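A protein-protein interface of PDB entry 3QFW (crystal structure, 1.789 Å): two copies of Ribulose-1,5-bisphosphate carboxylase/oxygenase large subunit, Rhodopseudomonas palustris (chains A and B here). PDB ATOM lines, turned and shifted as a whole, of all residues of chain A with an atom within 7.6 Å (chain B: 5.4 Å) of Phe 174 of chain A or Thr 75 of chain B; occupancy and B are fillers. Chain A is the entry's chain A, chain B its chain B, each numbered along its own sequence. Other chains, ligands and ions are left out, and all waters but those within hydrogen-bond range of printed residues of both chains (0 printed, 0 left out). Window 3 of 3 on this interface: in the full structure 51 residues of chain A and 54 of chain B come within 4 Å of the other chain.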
ATOM      1  N   PRO A 140      29.468   8.038  -1.801  1.00  0.00           N
ATOM      2  CA  PRO A 140      29.039   8.674  -0.554  1.00  0.00           C
ATOM      3  C   PRO A 140      27.641   8.246  -0.131  1.00  0.00           C
ATOM      4  O   PRO A 140      26.814   7.849  -0.946  1.00  0.00           O
ATOM      5  CB  PRO A 140      29.041  10.163  -0.912  1.00  0.00           C
ATOM      6  CG  PRO A 140      28.709  10.181  -2.377  1.00  0.00           C
ATOM      7  CD  PRO A 140      29.318   8.931  -2.965  1.00  0.00           C
ATOM      8  N   GLN A 141      27.399   8.327   1.169  1.00  0.00           N
ATOM      9  CA  GLN A 141      26.077   8.158   1.726  1.00  0.00           C
ATOM     10  C   GLN A 141      25.164   9.190   1.069  1.00  0.00           C
ATOM     11  O   GLN A 141      25.590  10.313   0.800  1.00  0.00           O
ATOM     12  CB  GLN A 141      26.148   8.427   3.224  1.00  0.00           C
ATOM     13  CG  GLN A 141      24.967   7.961   3.989  1.00  0.00           C
ATOM     14  CD  GLN A 141      24.908   8.601   5.359  1.00  0.00           C
ATOM     15  OE1 GLN A 141      23.832   8.899   5.856  1.00  0.00           O
ATOM     16  NE2 GLN A 141      26.068   8.822   5.970  1.00  0.00           N
ATOM     17  N   GLY A 142      23.919   8.813   0.805  1.00  0.00           N
ATOM     18  CA  GLY A 142      22.981   9.731   0.181  1.00  0.00           C
ATOM     19  C   GLY A 142      22.635   9.332  -1.241  1.00  0.00           C
ATOM     20  O   GLY A 142      21.694   9.864  -1.834  1.00  0.00           O
ATOM     21  N   LEU A 143      23.399   8.391  -1.788  1.00  0.00           N
ATOM     22  CA  LEU A 143      23.110   7.829  -3.104  1.00  0.00           C
ATOM     23  C   LEU A 143      21.952   6.852  -2.985  1.00  0.00           C
ATOM     24  O   LEU A 143      21.699   6.308  -1.914  1.00  0.00           O
ATOM     25  CB  LEU A 143      24.339   7.097  -3.663  1.00  0.00           C
ATOM     26  CG  LEU A 143      25.479   7.928  -4.258  1.00  0.00           C
ATOM     27  CD1 LEU A 143      26.733   7.081  -4.428  1.00  0.00           C
ATOM     28  CD2 LEU A 143      25.054   8.550  -5.584  1.00  0.00           C
ATOM     29  N   SER A 144      21.251   6.622  -4.087  1.00  0.00           N
ATOM     30  CA  SER A 144      20.182   5.637  -4.094  1.00  0.00           C
ATOM     31  C   SER A 144      20.796   4.247  -4.059  1.00  0.00           C
ATOM     32  O   SER A 144      21.968   4.072  -4.393  1.00  0.00           O
ATOM     33  CB  SER A 144      19.339   5.784  -5.358  1.00  0.00           C
ATOM     34  OG  SER A 144      20.093   5.383  -6.490  1.00  0.00           O
ATOM     35  N   PRO A 145      20.007   3.248  -3.645  1.00  0.00           N
ATOM     36  CA  PRO A 145      20.451   1.850  -3.683  1.00  0.00           C
ATOM     37  C   PRO A 145      20.997   1.449  -5.054  1.00  0.00           C
ATOM     38  O   PRO A 145      21.958   0.670  -5.136  1.00  0.00           O
ATOM     39  CB  PRO A 145      19.166   1.080  -3.368  1.00  0.00           C
ATOM     40  CG  PRO A 145      18.403   2.007  -2.494  1.00  0.00           C
ATOM     41  CD  PRO A 145      18.672   3.386  -3.038  1.00  0.00           C
ATOM     42  N   ALA A 146      20.402   1.976  -6.121  1.00  0.00           N
ATOM     43  CA  ALA A 146      20.848   1.628  -7.465  1.00  0.00           C
ATOM     44  C   ALA A 146      22.229   2.202  -7.776  1.00  0.00           C
ATOM     45  O   ALA A 146      23.085   1.516  -8.351  1.00  0.00           O
ATOM     46  CB  ALA A 146      19.829   2.079  -8.504  1.00  0.00           C
ATOM     47  N   LEU A 148      24.477   3.043  -5.551  1.00  0.00           N
ATOM     48  CA  LEU A 148      25.391   2.294  -4.687  1.00  0.00           C
ATOM     49  C   LEU A 148      25.691   0.944  -5.332  1.00  0.00           C
ATOM     50  O   LEU A 148      26.853   0.521  -5.440  1.00  0.00           O
ATOM     51  CB  LEU A 148      24.778   2.092  -3.292  1.00  0.00           C
ATOM     52  CG  LEU A 148      24.546   3.329  -2.411  1.00  0.00           C
ATOM     53  CD1 LEU A 148      23.661   2.993  -1.209  1.00  0.00           C
ATOM     54  CD2 LEU A 148      25.866   3.952  -1.960  1.00  0.00           C
ATOM     55  N   GLY A 168      28.533   4.833   7.935  1.00  0.00           N
ATOM     56  CA  GLY A 168      27.486   5.814   8.122  1.00  0.00           C
ATOM     57  C   GLY A 168      26.163   5.403   7.514  1.00  0.00           C
ATOM     58  O   GLY A 168      25.130   5.977   7.829  1.00  0.00           O
ATOM     59  N   LEU A 169      26.191   4.409   6.632  1.00  0.00           N
ATOM     60  CA  LEU A 169      24.966   3.909   6.024  1.00  0.00           C
ATOM     61  C   LEU A 169      24.229   3.024   7.016  1.00  0.00           C
ATOM     62  O   LEU A 169      24.792   2.073   7.562  1.00  0.00           O
ATOM     63  CB  LEU A 169      25.257   3.139   4.726  1.00  0.00           C
ATOM     64  CG  LEU A 169      25.533   3.936   3.449  1.00  0.00           C
ATOM     65  CD1 LEU A 169      26.193   3.050   2.392  1.00  0.00           C
ATOM     66  CD2 LEU A 169      24.254   4.574   2.897  1.00  0.00           C
ATOM     67  N   ALA A 170      22.964   3.349   7.252  1.00  0.00           N
ATOM     68  CA  ALA A 170      22.140   2.575   8.165  1.00  0.00           C
ATOM     69  C   ALA A 170      20.803   2.264   7.517  1.00  0.00           C
ATOM     70  O   ALA A 170      20.717   1.414   6.640  1.00  0.00           O
ATOM     71  CB  ALA A 170      21.945   3.329   9.501  1.00  0.00           C
ATOM     72  N   ASP A 171      19.758   2.965   7.935  1.00  0.00           N
ATOM     73  CA  ASP A 171      18.425   2.693   7.409  1.00  0.00           C
ATOM     74  C   ASP A 171      17.722   3.994   7.013  1.00  0.00           C
ATOM     75  O   ASP A 171      16.510   4.131   7.158  1.00  0.00           O
ATOM     76  CB  ASP A 171      17.618   1.903   8.441  1.00  0.00           C
ATOM     77  CG  ASP A 171      16.409   1.207   7.845  1.00  0.00           C
ATOM     78  OD1 ASP A 171      16.365   1.013   6.608  1.00  0.00           O
ATOM     79  OD2 ASP A 171      15.505   0.841   8.629  1.00  0.00           O
ATOM     80  N   GLN A 172      18.500   4.939   6.488  1.00  0.00           N
ATOM     81  CA  GLN A 172      17.971   6.234   6.078  1.00  0.00           C
ATOM     82  C   GLN A 172      17.008   6.152   4.901  1.00  0.00           C
ATOM     83  O   GLN A 172      17.067   5.226   4.093  1.00  0.00           O
ATOM     84  CB  GLN A 172      19.112   7.194   5.729  1.00  0.00           C
ATOM     85  CG  GLN A 172      20.104   7.421   6.855  1.00  0.00           C
ATOM     86  CD  GLN A 172      21.321   6.517   6.736  1.00  0.00           C
ATOM     87  OE1 GLN A 172      21.220   5.376   6.292  1.00  0.00           O
ATOM     88  NE2 GLN A 172      22.480   7.038   7.114  1.00  0.00           N
ATOM     89  N   ALA A 173      16.137   7.150   4.797  1.00  0.00           N
ATOM     90  CA  ALA A 173      15.145   7.195   3.727  1.00  0.00           C
ATOM     91  C   ALA A 173      15.775   7.115   2.345  1.00  0.00           C
ATOM     92  O   ALA A 173      15.262   6.417   1.469  1.00  0.00           O
ATOM     93  CB  ALA A 173      14.290   8.460   3.847  1.00  0.00           C
ATOM     94  N   PHE A 174      16.883   7.827   2.147  1.00  0.00           N
ATOM     95  CA  PHE A 174      17.496   7.909   0.827  1.00  0.00           C
ATOM     96  C   PHE A 174      18.076   6.578   0.327  1.00  0.00           C
ATOM     97  O   PHE A 174      18.409   6.443  -0.855  1.00  0.00           O
ATOM     98  CB  PHE A 174      18.538   9.039   0.755  1.00  0.00           C
ATOM     99  CG  PHE A 174      19.576   9.000   1.850  1.00  0.00           C
ATOM    100  CD1 PHE A 174      20.384   7.882   2.030  1.00  0.00           C
ATOM    101  CD2 PHE A 174      19.781  10.099   2.661  1.00  0.00           C
ATOM    102  CE1 PHE A 174      21.349   7.858   3.029  1.00  0.00           C
ATOM    103  CE2 PHE A 174      20.745  10.081   3.658  1.00  0.00           C
ATOM    104  CZ  PHE A 174      21.530   8.957   3.841  1.00  0.00           C
ATOM    105  N   SER A 175      18.186   5.600   1.222  1.00  0.00           N
ATOM    106  CA  SER A 175      18.679   4.273   0.836  1.00  0.00           C
ATOM    107  C   SER A 175      18.484   3.263   1.961  1.00  0.00           C
ATOM    108  O   SER A 175      19.449   2.844   2.599  1.00  0.00           O
ATOM    109  CB  SER A 175      20.153   4.322   0.394  1.00  0.00           C
ATOM    110  OG  SER A 175      21.036   4.514   1.490  1.00  0.00           O
ATOM    111  N   PRO A 176      17.225   2.867   2.203  1.00  0.00           N
ATOM    112  CA  PRO A 176      16.818   1.973   3.296  1.00  0.00           C
ATOM    113  C   PRO A 176      17.596   0.661   3.287  1.00  0.00           C
ATOM    114  O   PRO A 176      17.940   0.198   2.213  1.00  0.00           O
ATOM    115  CB  PRO A 176      15.344   1.700   2.984  1.00  0.00           C
ATOM    116  CG  PRO A 176      14.893   2.918   2.236  1.00  0.00           C
ATOM    117  CD  PRO A 176      16.075   3.308   1.391  1.00  0.00           C
ATOM    118  N   GLU A 179      16.313  -2.184   0.839  1.00  0.00           N
ATOM    119  CA  GLU A 179      16.478  -1.825  -0.567  1.00  0.00           C
ATOM    120  C   GLU A 179      17.946  -1.782  -0.996  1.00  0.00           C
ATOM    121  O   GLU A 179      18.283  -2.146  -2.126  1.00  0.00           O
ATOM    122  CB  GLU A 179      15.783  -0.494  -0.871  1.00  0.00           C
ATOM    123  CG  GLU A 179      14.276  -0.622  -1.052  1.00  0.00           C
ATOM    124  CD  GLU A 179      13.605  -1.298   0.125  1.00  0.00           C
ATOM    125  OE1 GLU A 179      12.901  -2.313  -0.086  1.00  0.00           O
ATOM    126  OE2 GLU A 179      13.785  -0.817   1.265  1.00  0.00           O
ATOM    127  N   ARG A 180      18.816  -1.341  -0.094  1.00  0.00           N
ATOM    128  CA  ARG A 180      20.251  -1.276  -0.385  1.00  0.00           C
ATOM    129  C   ARG A 180      20.865  -2.674  -0.483  1.00  0.00           C
ATOM    130  O   ARG A 180      21.566  -2.999  -1.456  1.00  0.00           O
ATOM    131  CB  ARG A 180      20.969  -0.478   0.705  1.00  0.00           C
ATOM    132  CG  ARG A 180      22.454  -0.270   0.472  1.00  0.00           C
ATOM    133  CD  ARG A 180      23.127   0.213   1.752  1.00  0.00           C
ATOM    134  NE  ARG A 180      22.304   1.190   2.453  1.00  0.00           N
ATOM    135  CZ  ARG A 180      22.125   1.218   3.769  1.00  0.00           C
ATOM    136  NH1 ARG A 180      22.722   0.325   4.554  1.00  0.00           N
ATOM    137  NH2 ARG A 180      21.357   2.150   4.302  1.00  0.00           N
ATOM    138  N   GLN B  32      32.232  13.558   9.352  1.00  0.00           N
ATOM    139  CA  GLN B  32      30.935  13.275   9.963  1.00  0.00           C
ATOM    140  C   GLN B  32      29.814  13.391   8.946  1.00  0.00           C
ATOM    141  O   GLN B  32      28.648  13.584   9.290  1.00  0.00           O
ATOM    142  CB  GLN B  32      30.678  14.204  11.145  1.00  0.00           C
ATOM    143  CG  GLN B  32      31.675  14.026  12.285  1.00  0.00           C
ATOM    144  CD  GLN B  32      31.843  12.567  12.693  1.00  0.00           C
ATOM    145  OE1 GLN B  32      32.940  12.131  13.016  1.00  0.00           O
ATOM    146  NE2 GLN B  32      30.748  11.818  12.695  1.00  0.00           N
ATOM    147  N   ILE B  50      24.128  16.887   1.445  1.00  0.00           N
ATOM    148  CA  ILE B  50      24.572  15.832   2.354  1.00  0.00           C
ATOM    149  C   ILE B  50      25.923  16.114   3.012  1.00  0.00           C
ATOM    150  O   ILE B  50      26.097  15.859   4.202  1.00  0.00           O
ATOM    151  CB  ILE B  50      24.621  14.462   1.652  1.00  0.00           C
ATOM    152  CG1 ILE B  50      23.245  14.113   1.081  1.00  0.00           C
ATOM    153  CG2 ILE B  50      25.108  13.383   2.613  1.00  0.00           C
ATOM    154  CD1 ILE B  50      22.126  14.273   2.060  1.00  0.00           C
ATOM    155  N   LEU B  71      24.782  19.447   9.904  1.00  0.00           N
ATOM    156  CA  LEU B  71      24.731  18.090   9.373  1.00  0.00           C
ATOM    157  C   LEU B  71      23.350  17.790   8.813  1.00  0.00           C
ATOM    158  O   LEU B  71      22.350  17.978   9.495  1.00  0.00           O
ATOM    159  CB  LEU B  71      25.082  17.065  10.458  1.00  0.00           C
ATOM    160  CG  LEU B  71      26.508  17.077  11.027  1.00  0.00           C
ATOM    161  CD1 LEU B  71      26.655  16.079  12.176  1.00  0.00           C
ATOM    162  CD2 LEU B  71      27.535  16.787   9.943  1.00  0.00           C
ATOM    163  N   ALA B  72      23.294  17.328   7.565  1.00  0.00           N
ATOM    164  CA  ALA B  72      22.016  16.976   6.954  1.00  0.00           C
ATOM    165  C   ALA B  72      21.238  15.996   7.827  1.00  0.00           C
ATOM    166  O   ALA B  72      21.735  14.914   8.145  1.00  0.00           O
ATOM    167  CB  ALA B  72      22.224  16.398   5.573  1.00  0.00           C
ATOM    168  N   ALA B  73      20.027  16.383   8.223  1.00  0.00           N
ATOM    169  CA  ALA B  73      19.164  15.505   9.014  1.00  0.00           C
ATOM    170  C   ALA B  73      18.889  14.167   8.325  1.00  0.00           C
ATOM    171  O   ALA B  73      18.631  13.161   8.990  1.00  0.00           O
ATOM    172  CB  ALA B  73      17.848  16.202   9.344  1.00  0.00           C
ATOM    173  N   ALA B  74      18.921  14.164   6.997  1.00  0.00           N
ATOM    174  CA  ALA B  74      18.643  12.949   6.236  1.00  0.00           C
ATOM    175  C   ALA B  74      19.585  11.827   6.651  1.00  0.00           C
ATOM    176  O   ALA B  74      19.202  10.662   6.663  1.00  0.00           O
ATOM    177  CB  ALA B  74      18.763  13.212   4.744  1.00  0.00           C
ATOM    178  N   THR B  75      20.815  12.194   6.998  1.00  0.00           N
ATOM    179  CA  THR B  75      21.842  11.206   7.321  1.00  0.00           C
ATOM    180  C   THR B  75      21.610  10.565   8.688  1.00  0.00           C
ATOM    181  O   THR B  75      22.082   9.453   8.950  1.00  0.00           O
ATOM    182  CB  THR B  75      23.254  11.819   7.262  1.00  0.00           C
ATOM    183  OG1 THR B  75      23.444  12.723   8.356  1.00  0.00           O
ATOM    184  CG2 THR B  75      23.448  12.570   5.961  1.00  0.00           C
ATOM    185  N   ALA B  76      20.878  11.252   9.563  1.00  0.00           N
ATOM    186  CA  ALA B  76      20.652  10.706  10.898  1.00  0.00           C
ATOM    187  C   ALA B  76      19.185  10.721  11.342  1.00  0.00           C
ATOM    188  O   ALA B  76      18.706  11.703  11.931  1.00  0.00           O
ATOM    189  CB  ALA B  76      21.540  11.419  11.907  1.00  0.00           C
ATOM    190  N   PRO B  77      18.472   9.613  11.084  1.00  0.00           N
ATOM    191  CA  PRO B  77      17.081   9.439  11.501  1.00  0.00           C
ATOM    192  C   PRO B  77      16.993   9.472  13.025  1.00  0.00           C
ATOM    193  O   PRO B  77      18.025   9.366  13.691  1.00  0.00           O
ATOM    194  CB  PRO B  77      16.729   8.030  10.989  1.00  0.00           C
ATOM    195  CG  PRO B  77      17.821   7.641  10.077  1.00  0.00           C
ATOM    196  CD  PRO B  77      19.034   8.365  10.551  1.00  0.00           C
ATOM    197  N   GLN B  82      22.319   5.574  15.588  1.00  0.00           N
ATOM    198  CA  GLN B  82      22.670   6.211  14.320  1.00  0.00           C
ATOM    199  C   GLN B  82      22.924   7.702  14.468  1.00  0.00           C
ATOM    200  O   GLN B  82      23.795   8.264  13.798  1.00  0.00           O
ATOM    201  CB  GLN B  82      21.593   5.955  13.266  1.00  0.00           C
ATOM    202  CG  GLN B  82      21.862   6.612  11.908  1.00  0.00           C
ATOM    203  CD  GLN B  82      23.124   6.099  11.205  1.00  0.00           C
ATOM    204  OE1 GLN B  82      23.754   5.134  11.641  1.00  0.00           O
ATOM    205  NE2 GLN B  82      23.498   6.761  10.116  1.00  0.00           N
ATOM    206  N   MET B  86      26.383   9.475  13.505  1.00  0.00           N
ATOM    207  CA  MET B  86      26.610  10.637  12.648  1.00  0.00           C
ATOM    208  C   MET B  86      27.208  11.829  13.417  1.00  0.00           C
ATOM    209  O   MET B  86      27.966  12.623  12.849  1.00  0.00           O
ATOM    210  CB  MET B  86      25.325  11.054  11.905  1.00  0.00           C
ATOM    211  CG  MET B  86      24.911  10.150  10.709  1.00  0.00           C
ATOM    212  SD  MET B  86      26.216   9.302   9.745  1.00  0.00           S
ATOM    213  CE  MET B  86      26.141   7.702  10.492  1.00  0.00           C
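Gln 141 of chain A touches Ile 50 of chain B.
Thr 75 of chain B touches Gln 141 of chain A.
NE2 of Gln 141 of chain A touches SD of Met 86 of chain B, at 3.8 Å.
Met 86 of chain B touches Gly 168 of chain A.
Ala 170 of chain A touches Gln 82 of chain B.
Gln 172 of chain A touches Ala 74 of chain B (CG to O, 3.4 Å).
CG of Pro 77 of chain B touches CG of Gln 172 of chain A, 3.95 Å away.
Phe 174 of chain A touches Ala 74 of chain B.
CE2 of Phe 174 of chain A touches N of Thr 75 of chain B, 3.95 Å away.
No position is printed for both chains.
Printed residues of chain B within 4 Å of Gly 168 of chain A: Gln 82 (2.9 Å) and Met 86 (3.3 Å).
Phe 174 of chain A touches just these residues of chain B: Ala 74 (3.4 Å) and Thr 75 (3.95 Å).
Printed residues of chain A within 4 Å of Ile 50 of chain B: Gln 141 (3.6 Å).
Thr 75 of chain B touches three residues of chain A.
Of the printed residues of chain A, Pro 77 of chain B touches Gln 172 (3.95 Å).
The nearest residue of chain B that does not touch Phe 174 of chain A is Ile 50 of chain B (4.7 Å).
NE2 of Gln 172 of chain A is in hydrogen-bond range of O of Gly 168 of chain A, at 2.9 Å.
The backbone NH (N) of Ala 170 of chain A is in hydrogen-bond range of the side-chain amide oxygen (OE1) of Gln 172 of chain A, 2.8 Å away.
The guanidinium group (NH2) of Arg 180 of chain A lies within hydrogen-bond range of the backbone carbonyl oxygen (O) of Ala 170 of chain A.
The backbone carbonyl oxygen of Ala 72 of chain B is in hydrogen-bond range of the side-chain hydroxyl of Thr 75 of chain B (2.8 Å).
The backbone carbonyl oxygen (O) of Thr 75 of chain B sits at hydrogen-bond distance from the side-chain amide nitrogen (NE2) of Gln 82 of chain B (3.3 Å).
The side-chain amide nitrogen (NE2) of Gln 82 of chain B sits close to the side-chain sulfur (SD) of Met 86 of chain B (3.7 Å).
Of the 19 printed residues of chain A, 5 touch a printed residue of chain B.
Hydrophobic or aromatic side chains of chain A that line the printed part of chain B: Ala 170 and Phe 174.
Along chain A the printed residues that touch a printed residue of chain B span positions 141 to 174.
Among the printed residues, 12 pairs touch across the chains.
Among the printed residues, no Asp or Glu carboxylate lies within 4 Å of a Lys or Arg side-chain nitrogen of the other chain.
The side-chain amide nitrogen of Gln 82 of chain B is in hydrogen-bond range of the backbone carbonyl oxygen of Gly 168 of chain A.
The side-chain amide nitrogen of Gln 172 of chain A lies within hydrogen-bond range of the backbone carbonyl oxygen of Thr 75 of chain B (3.1 Å).
NE2 of Gln 172 of chain A lies close to NE2 of Gln 82 of chain B (3.2 Å).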
